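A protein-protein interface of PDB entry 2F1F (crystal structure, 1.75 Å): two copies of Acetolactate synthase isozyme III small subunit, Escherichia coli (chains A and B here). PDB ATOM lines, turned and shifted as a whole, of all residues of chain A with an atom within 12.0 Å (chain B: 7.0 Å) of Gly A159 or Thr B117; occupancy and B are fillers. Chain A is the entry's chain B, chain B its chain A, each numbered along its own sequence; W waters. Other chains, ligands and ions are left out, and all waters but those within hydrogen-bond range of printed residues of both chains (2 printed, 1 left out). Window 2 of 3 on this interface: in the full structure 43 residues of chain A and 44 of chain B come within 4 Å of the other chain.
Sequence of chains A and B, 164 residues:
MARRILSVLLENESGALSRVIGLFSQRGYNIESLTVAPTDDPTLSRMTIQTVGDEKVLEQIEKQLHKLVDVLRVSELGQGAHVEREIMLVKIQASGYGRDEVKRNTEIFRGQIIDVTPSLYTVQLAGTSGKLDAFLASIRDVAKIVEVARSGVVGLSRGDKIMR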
ATOM      1  N   LEU A  77     -11.276  -0.937   6.682  1.00  0.00           N
ATOM      2  CA  LEU A  77     -10.936  -1.868   5.587  1.00  0.00           C
ATOM      3  C   LEU A  77     -11.968  -2.991   5.437  1.00  0.00           C
ATOM      4  O   LEU A  77     -12.398  -3.323   4.309  1.00  0.00           O
ATOM      5  CB  LEU A  77      -9.527  -2.434   5.785  1.00  0.00           C
ATOM      6  CG  LEU A  77      -8.457  -1.605   5.048  1.00  0.00           C
ATOM      7  CD1 LEU A  77      -7.140  -1.410   5.821  1.00  0.00           C
ATOM      8  CD2 LEU A  77      -8.220  -2.248   3.686  1.00  0.00           C
ATOM      9  N   GLN A  79     -14.886  -3.190   5.196  1.00  0.00           N
ATOM     10  CA  GLN A  79     -16.112  -2.757   4.536  1.00  0.00           C
ATOM     11  C   GLN A  79     -16.033  -3.018   3.030  1.00  0.00           C
ATOM     12  O   GLN A  79     -16.984  -2.740   2.291  1.00  0.00           O
ATOM     13  CB  GLN A  79     -16.406  -1.283   4.836  1.00  0.00           C
ATOM     14  CG  GLN A  79     -16.883  -1.076   6.284  1.00  0.00           C
ATOM     15  CD  GLN A  79     -18.191  -0.294   6.395  1.00  0.00           C
ATOM     16  OE1 GLN A  79     -19.048  -0.352   5.503  1.00  0.00           O
ATOM     17  NE2 GLN A  79     -18.358   0.426   7.508  1.00  0.00           N
ATOM     18  N   GLY A  80     -14.880  -3.529   2.595  1.00  0.00           N
ATOM     19  CA  GLY A  80     -14.744  -4.192   1.280  1.00  0.00           C
ATOM     20  C   GLY A  80     -14.810  -5.696   1.477  1.00  0.00           C
ATOM     21  O   GLY A  80     -14.711  -6.145   2.619  1.00  0.00           O
ATOM     22  N   ALA A  81     -14.865  -6.509   0.418  1.00  0.00           N
ATOM     23  CA  ALA A  81     -14.400  -6.175  -0.942  1.00  0.00           C
ATOM     24  C   ALA A  81     -13.023  -5.503  -0.789  1.00  0.00           C
ATOM     25  O   ALA A  81     -12.826  -4.311  -1.050  1.00  0.00           O
ATOM     26  CB  ALA A  81     -15.373  -5.298  -1.693  1.00  0.00           C
ATOM     27  N   HIS A  82     -12.073  -6.286  -0.316  1.00  0.00           N
ATOM     28  CA  HIS A  82     -10.750  -5.715  -0.049  1.00  0.00           C
ATOM     29  C   HIS A  82      -9.636  -6.755  -0.116  1.00  0.00           C
ATOM     30  O   HIS A  82      -9.894  -7.973  -0.102  1.00  0.00           O
ATOM     31  CB  HIS A  82     -10.748  -5.103   1.340  1.00  0.00           C
ATOM     32  CG  HIS A  82     -10.848  -6.123   2.428  1.00  0.00           C
ATOM     33  ND1 HIS A  82     -12.049  -6.659   2.839  1.00  0.00           N
ATOM     34  CD2 HIS A  82      -9.890  -6.731   3.172  1.00  0.00           C
ATOM     35  CE1 HIS A  82     -11.826  -7.545   3.798  1.00  0.00           C
ATOM     36  NE2 HIS A  82     -10.528  -7.603   4.021  1.00  0.00           N
ATOM     37  N   VAL A  83      -8.404  -6.260  -0.221  1.00  0.00           N
ATOM     38  CA  VAL A  83      -7.229  -7.140  -0.056  1.00  0.00           C
ATOM     39  C   VAL A  83      -6.420  -6.686   1.189  1.00  0.00           C
ATOM     40  O   VAL A  83      -6.254  -5.503   1.402  1.00  0.00           O
ATOM     41  CB  VAL A  83      -6.327  -7.135  -1.316  1.00  0.00           C
ATOM     42  CG1 VAL A  83      -7.025  -7.872  -2.474  1.00  0.00           C
ATOM     43  CG2 VAL A  83      -5.918  -5.692  -1.756  1.00  0.00           C
ATOM     44  N   GLU A  84      -5.916  -7.613   1.995  1.00  0.00           N
ATOM     45  CA  GLU A  84      -5.125  -7.262   3.196  1.00  0.00           C
ATOM     46  C   GLU A  84      -3.902  -8.168   3.189  1.00  0.00           C
ATOM     47  O   GLU A  84      -4.029  -9.369   2.967  1.00  0.00           O
ATOM     48  CB  GLU A  84      -5.888  -7.531   4.512  1.00  0.00           C
ATOM     49  CG  GLU A  84      -6.257  -9.011   4.628  1.00  0.00           C
ATOM     50  CD  GLU A  84      -5.919  -9.702   5.976  1.00  0.00           C
ATOM     51  OE1 GLU A  84      -6.619  -9.345   6.988  1.00  0.00           O
ATOM     52  OE2 GLU A  84      -5.025 -10.650   5.985  1.00  0.00           O
ATOM     53  N   GLY A 155      -3.792  -2.685   3.781  1.00  0.00           N
ATOM     54  CA  GLY A 155      -4.794  -3.093   2.798  1.00  0.00           C
ATOM     55  C   GLY A 155      -5.359  -2.050   1.889  1.00  0.00           C
ATOM     56  O   GLY A 155      -5.142  -0.877   2.101  1.00  0.00           O
ATOM     57  N   LEU A 156      -6.044  -2.526   0.852  1.00  0.00           N
ATOM     58  CA  LEU A 156      -6.724  -1.677  -0.149  1.00  0.00           C
ATOM     59  C   LEU A 156      -8.093  -2.279  -0.569  1.00  0.00           C
ATOM     60  O   LEU A 156      -8.297  -3.462  -0.528  1.00  0.00           O
ATOM     61  CB  LEU A 156      -5.881  -1.536  -1.430  1.00  0.00           C
ATOM     62  CG  LEU A 156      -4.501  -0.881  -1.517  1.00  0.00           C
ATOM     63  CD1 LEU A 156      -4.086  -1.072  -2.924  1.00  0.00           C
ATOM     64  CD2 LEU A 156      -4.507   0.575  -1.144  1.00  0.00           C
ATOM     65  N   SER A 157      -9.028  -1.461  -1.026  1.00  0.00           N
ATOM     66  CA  SER A 157     -10.260  -2.049  -1.574  1.00  0.00           C
ATOM     67  C   SER A 157      -9.961  -2.778  -2.884  1.00  0.00           C
ATOM     68  O   SER A 157      -9.017  -2.427  -3.590  1.00  0.00           O
ATOM     69  CB  SER A 157     -11.260  -0.958  -1.900  1.00  0.00           C
ATOM     70  OG  SER A 157     -10.642  -0.013  -2.808  1.00  0.00           O
ATOM     71  N   ARG A 158     -10.790  -3.746  -3.239  1.00  0.00           N
ATOM     72  CA  ARG A 158     -10.703  -4.293  -4.591  1.00  0.00           C
ATOM     73  C   ARG A 158     -11.196  -3.279  -5.652  1.00  0.00           C
ATOM     74  O   ARG A 158     -12.034  -2.420  -5.363  1.00  0.00           O
ATOM     75  CB  ARG A 158     -11.443  -5.630  -4.677  1.00  0.00           C
ATOM     76  CG  ARG A 158     -10.708  -6.725  -3.997  1.00  0.00           C
ATOM     77  CD  ARG A 158     -11.006  -8.053  -4.642  1.00  0.00           C
ATOM     78  NE  ARG A 158     -10.398  -9.121  -3.852  1.00  0.00           N
ATOM     79  CZ  ARG A 158      -9.198  -9.652  -4.105  1.00  0.00           C
ATOM     80  NH1 ARG A 158      -8.465  -9.223  -5.147  1.00  0.00           N
ATOM     81  NH2 ARG A 158      -8.725 -10.615  -3.314  1.00  0.00           N
ATOM     82  N   GLY A 159     -10.677  -3.383  -6.872  1.00  0.00           N
ATOM     83  CA  GLY A 159     -11.113  -2.520  -7.971  1.00  0.00           C
ATOM     84  C   GLY A 159     -12.297  -3.046  -8.737  1.00  0.00           C
ATOM     85  O   GLY A 159     -13.070  -3.866  -8.227  1.00  0.00           O
ATOM     86  N   LYS B  91      -2.319   0.160  -6.209  1.00  0.00           N
ATOM     87  CA  LYS B  91      -3.361   0.092  -7.226  1.00  0.00           C
ATOM     88  C   LYS B  91      -2.976   1.017  -8.368  1.00  0.00           C
ATOM     89  O   LYS B  91      -2.738   2.223  -8.145  1.00  0.00           O
ATOM     90  CB  LYS B  91      -4.692   0.498  -6.632  1.00  0.00           C
ATOM     91  CG  LYS B  91      -5.855   0.399  -7.578  1.00  0.00           C
ATOM     92  CD  LYS B  91      -7.206   0.632  -6.886  1.00  0.00           C
ATOM     93  CE  LYS B  91      -7.558  -0.491  -5.908  1.00  0.00           C
ATOM     94  NZ  LYS B  91      -8.851  -0.308  -5.135  1.00  0.00           N
ATOM     95  N   ALA B  94      -4.021   1.529 -15.884  1.00  0.00           N
ATOM     96  CA  ALA B  94      -3.216   1.504 -17.132  1.00  0.00           C
ATOM     97  C   ALA B  94      -3.988   0.929 -18.308  1.00  0.00           C
ATOM     98  O   ALA B  94      -4.923   0.141 -18.141  1.00  0.00           O
ATOM     99  CB  ALA B  94      -1.922   0.686 -16.926  1.00  0.00           C
ATOM    100  N   ARG B  99      -0.133  -0.922 -19.610  1.00  0.00           N
ATOM    101  CA  ARG B  99      -0.472  -2.219 -18.964  1.00  0.00           C
ATOM    102  C   ARG B  99       0.741  -3.168 -19.147  1.00  0.00           C
ATOM    103  O   ARG B  99       1.162  -3.845 -18.222  1.00  0.00           O
ATOM    104  CB  ARG B  99      -1.693  -2.992 -19.530  1.00  0.00           C
ATOM    105  CG  ARG B  99      -3.073  -2.536 -19.320  1.00  0.00           C
ATOM    106  CD  ARG B  99      -3.678  -3.021 -18.047  1.00  0.00           C
ATOM    107  NE  ARG B  99      -4.524  -4.184 -18.139  1.00  0.00           N
ATOM    108  CZ  ARG B  99      -5.415  -4.459 -17.211  1.00  0.00           C
ATOM    109  NH1 ARG B  99      -5.544  -3.607 -16.171  1.00  0.00           N
ATOM    110  NH2 ARG B  99      -6.186  -5.543 -17.311  1.00  0.00           N
ATOM    111  N   ASP B 115      -4.932  -8.471  -7.884  1.00  0.00           N
ATOM    112  CA  ASP B 115      -6.312  -8.081  -8.268  1.00  0.00           C
ATOM    113  C   ASP B 115      -6.188  -7.510  -9.679  1.00  0.00           C
ATOM    114  O   ASP B 115      -5.231  -6.768  -9.939  1.00  0.00           O
ATOM    115  CB  ASP B 115      -6.873  -7.023  -7.278  1.00  0.00           C
ATOM    116  CG  ASP B 115      -8.391  -6.730  -7.447  1.00  0.00           C
ATOM    117  OD1 ASP B 115      -9.196  -7.658  -7.592  1.00  0.00           O
ATOM    118  OD2 ASP B 115      -8.796  -5.543  -7.359  1.00  0.00           O
ATOM    119  N   VAL B 116      -7.148  -7.776 -10.542  1.00  0.00           N
ATOM    120  CA  VAL B 116      -7.122  -7.381 -11.982  1.00  0.00           C
ATOM    121  C   VAL B 116      -8.481  -7.073 -12.467  1.00  0.00           C
ATOM    122  O   VAL B 116      -9.383  -7.911 -12.336  1.00  0.00           O
ATOM    123  CB  VAL B 116      -6.671  -8.548 -12.997  1.00  0.00           C
ATOM    124  CG1 VAL B 116      -6.521  -7.955 -14.474  1.00  0.00           C
ATOM    125  CG2 VAL B 116      -5.533  -9.339 -12.535  1.00  0.00           C
ATOM    126  N   THR B 117      -8.671  -5.888 -12.994  1.00  0.00           N
ATOM    127  CA  THR B 117      -9.861  -5.581 -13.735  1.00  0.00           C
ATOM    128  C   THR B 117      -9.374  -5.117 -15.118  1.00  0.00           C
ATOM    129  O   THR B 117      -8.163  -4.918 -15.344  1.00  0.00           O
ATOM    130  CB  THR B 117     -10.689  -4.491 -13.037  1.00  0.00           C
ATOM    131  OG1 THR B 117     -10.102  -3.236 -13.303  1.00  0.00           O
ATOM    132  CG2 THR B 117     -10.805  -4.741 -11.548  1.00  0.00           C
ATOM    133  N   PRO B 118     -10.318  -4.900 -16.079  1.00  0.00           N
ATOM    134  CA  PRO B 118      -9.800  -4.471 -17.350  1.00  0.00           C
ATOM    135  C   PRO B 118      -8.993  -3.170 -17.375  1.00  0.00           C
ATOM    136  O   PRO B 118      -8.219  -2.954 -18.330  1.00  0.00           O
ATOM    137  CB  PRO B 118     -11.072  -4.356 -18.258  1.00  0.00           C
ATOM    138  CG  PRO B 118     -12.172  -5.098 -17.532  1.00  0.00           C
ATOM    139  CD  PRO B 118     -11.761  -5.199 -16.081  1.00  0.00           C
ATOM    140  N   SER B 119      -9.131  -2.324 -16.349  1.00  0.00           N
ATOM    141  CA  SER B 119      -8.385  -1.077 -16.296  1.00  0.00           C
ATOM    142  C   SER B 119      -7.385  -0.932 -15.094  1.00  0.00           C
ATOM    143  O   SER B 119      -6.510  -0.045 -15.122  1.00  0.00           O
ATOM    144  CB  SER B 119      -9.420   0.080 -16.276  1.00  0.00           C
ATOM    145  OG  SER B 119     -10.212  -0.004 -15.088  1.00  0.00           O
ATOM    146  N   LEU B 120      -7.439  -1.848 -14.122  1.00  0.00           N
ATOM    147  CA  LEU B 120      -6.677  -1.698 -12.869  1.00  0.00           C
ATOM    148  C   LEU B 120      -5.882  -2.938 -12.545  1.00  0.00           C
ATOM    149  O   LEU B 120      -6.367  -4.086 -12.753  1.00  0.00           O
ATOM    150  CB  LEU B 120      -7.625  -1.447 -11.688  1.00  0.00           C
ATOM    151  CG  LEU B 120      -8.438  -0.149 -11.597  1.00  0.00           C
ATOM    152  CD1 LEU B 120      -9.378  -0.310 -10.391  1.00  0.00           C
ATOM    153  CD2 LEU B 120      -7.509   1.063 -11.455  1.00  0.00           C
ATOM    154  N   TYR B 121      -4.671  -2.749 -12.030  1.00  0.00           N
ATOM    155  CA  TYR B 121      -3.951  -3.837 -11.359  1.00  0.00           C
ATOM    156  C   TYR B 121      -3.651  -3.448  -9.907  1.00  0.00           C
ATOM    157  O   TYR B 121      -3.285  -2.309  -9.676  1.00  0.00           O
ATOM    158  CB  TYR B 121      -2.582  -4.029 -11.975  1.00  0.00           C
ATOM    159  CG  TYR B 121      -2.494  -4.673 -13.331  1.00  0.00           C
ATOM    160  CD1 TYR B 121      -3.408  -5.663 -13.773  1.00  0.00           C
ATOM    161  CD2 TYR B 121      -1.487  -4.259 -14.211  1.00  0.00           C
ATOM    162  CE1 TYR B 121      -3.252  -6.252 -15.069  1.00  0.00           C
ATOM    163  CE2 TYR B 121      -1.323  -4.859 -15.436  1.00  0.00           C
ATOM    164  CZ  TYR B 121      -2.181  -5.834 -15.859  1.00  0.00           C
ATOM    165  OH  TYR B 121      -1.909  -6.330 -17.118  1.00  0.00           O
ATOM    166  N   THR B 122      -3.713  -4.379  -8.984  1.00  0.00           N
ATOM    167  CA  THR B 122      -3.199  -4.191  -7.633  1.00  0.00           C
ATOM    168  C   THR B 122      -1.952  -5.036  -7.483  1.00  0.00           C
ATOM    169  O   THR B 122      -2.023  -6.253  -7.674  1.00  0.00           O
ATOM    170  CB  THR B 122      -4.221  -4.522  -6.561  1.00  0.00           C
ATOM    171  OG1 THR B 122      -5.340  -3.658  -6.774  1.00  0.00           O
ATOM    172  CG2 THR B 122      -3.615  -4.307  -5.152  1.00  0.00           C
HETATM  173  O   HOH W   1     -11.773  -6.570  -8.410  1.00  0.00           O
HETATM  174  O   HOH W   2      -7.265  -4.327  -4.949  1.00  0.00           O
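Among the printed residues, pairs that only touch across the chains: Gly A159 with Thr B117, Gly A159 with Leu B120, Arg A158 with Lys B91, Leu A156 with Lys B91, Leu A156 with Thr B122 and Gly A159 with Lys B91.
Gly A159 touches four residues of chain B.
Thr B117 touches one residue of chain A.
No residue of chain A comes within 4 Å of Val B116.
Pro B118 touches none of the printed residues of chain A.
Of the printed residues of chain A, Leu B120 touches Gly A159.
Printed residues of chain B within 4 Å of Ser A157: Lys B91 (2.6 Å).
Printed residues of chain A within 4 Å of Lys B91: Leu A156, Ser A157, Arg A158 and Gly A159.
Of the printed residues of chain B, Leu A156 touches Lys B91 (3.9 Å) and Thr B122 (3.96 Å).
Of the printed residues of chain B, Arg A158 touches Lys B91 and Asp B115.
Of the printed residues of chain A, Thr B122 touches Leu A156.
Leu A77 touches none of the printed residues of chain B.
The nearest residue of chain B that does not touch Gly A159 is Thr B122 (5.3 Å).
The nearest printed residue of chain A that does not touch Thr B122 is Val A83 (4.3 Å).
No position is printed for both chains.
Hydrophobic or aromatic side chains of chain B within 4 Å of the printed part of chain A: Leu B120.
Hydrophobic or aromatic side chains of chain A within 4 Å of the printed part of chain B: Leu A156.
Among the printed residues, 9 pairs touch across the chains.
Water W2 lies within hydrogen-bond range of the side-chain hydroxyl of Thr B122 (2.7 Å), the backbone carbonyl oxygen of Ser A157 (2.9 Å) and the side-chain carboxylate of Asp B115 (3.1 Å).
Water W1 lies within hydrogen-bond range of the side-chain carboxylate (OD1) of Asp B115 (2.9 Å) and the backbone carbonyl oxygen (O) of Gly A159 (3.0 Å).
The backbone carbonyl oxygen of Thr B117 sits at hydrogen-bond distance from the guanidinium group of Arg B99 (2.9 Å).
O of Asp B115 is in hydrogen-bond range of N of Thr B122, 3.0 Å away.
The side-chain hydroxyl (OG1) of Thr B117 lies close to the backbone NH (N) of Ser B119 (3.3 Å).
The side-chain hydroxyl (OG1) of Thr B117 lies within hydrogen-bond range of the backbone NH (N) of Leu B120 (3.1 Å).
The backbone carbonyl oxygen of Ala A81 lies within hydrogen-bond range of the backbone NH of Arg A158 (3.0 Å).
The backbone NH (N) of Val A83 sits at hydrogen-bond distance from the backbone carbonyl oxygen (O) of Leu A156 (2.8 Å).
The side-chain amino group of Lys B91 is in hydrogen-bond range of the backbone carbonyl oxygen of Ser A157 (2.6 Å).
The side-chain carboxylate (OD1) of Asp B115 lies within salt-bridge range of the guanidinium group (NH1) of Arg A158 (3.0 Å).
The side-chain carboxylate (OD2) of Asp B115 lies within hydrogen-bond range of the backbone NH (N) of Gly A159, at 2.9 Å.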
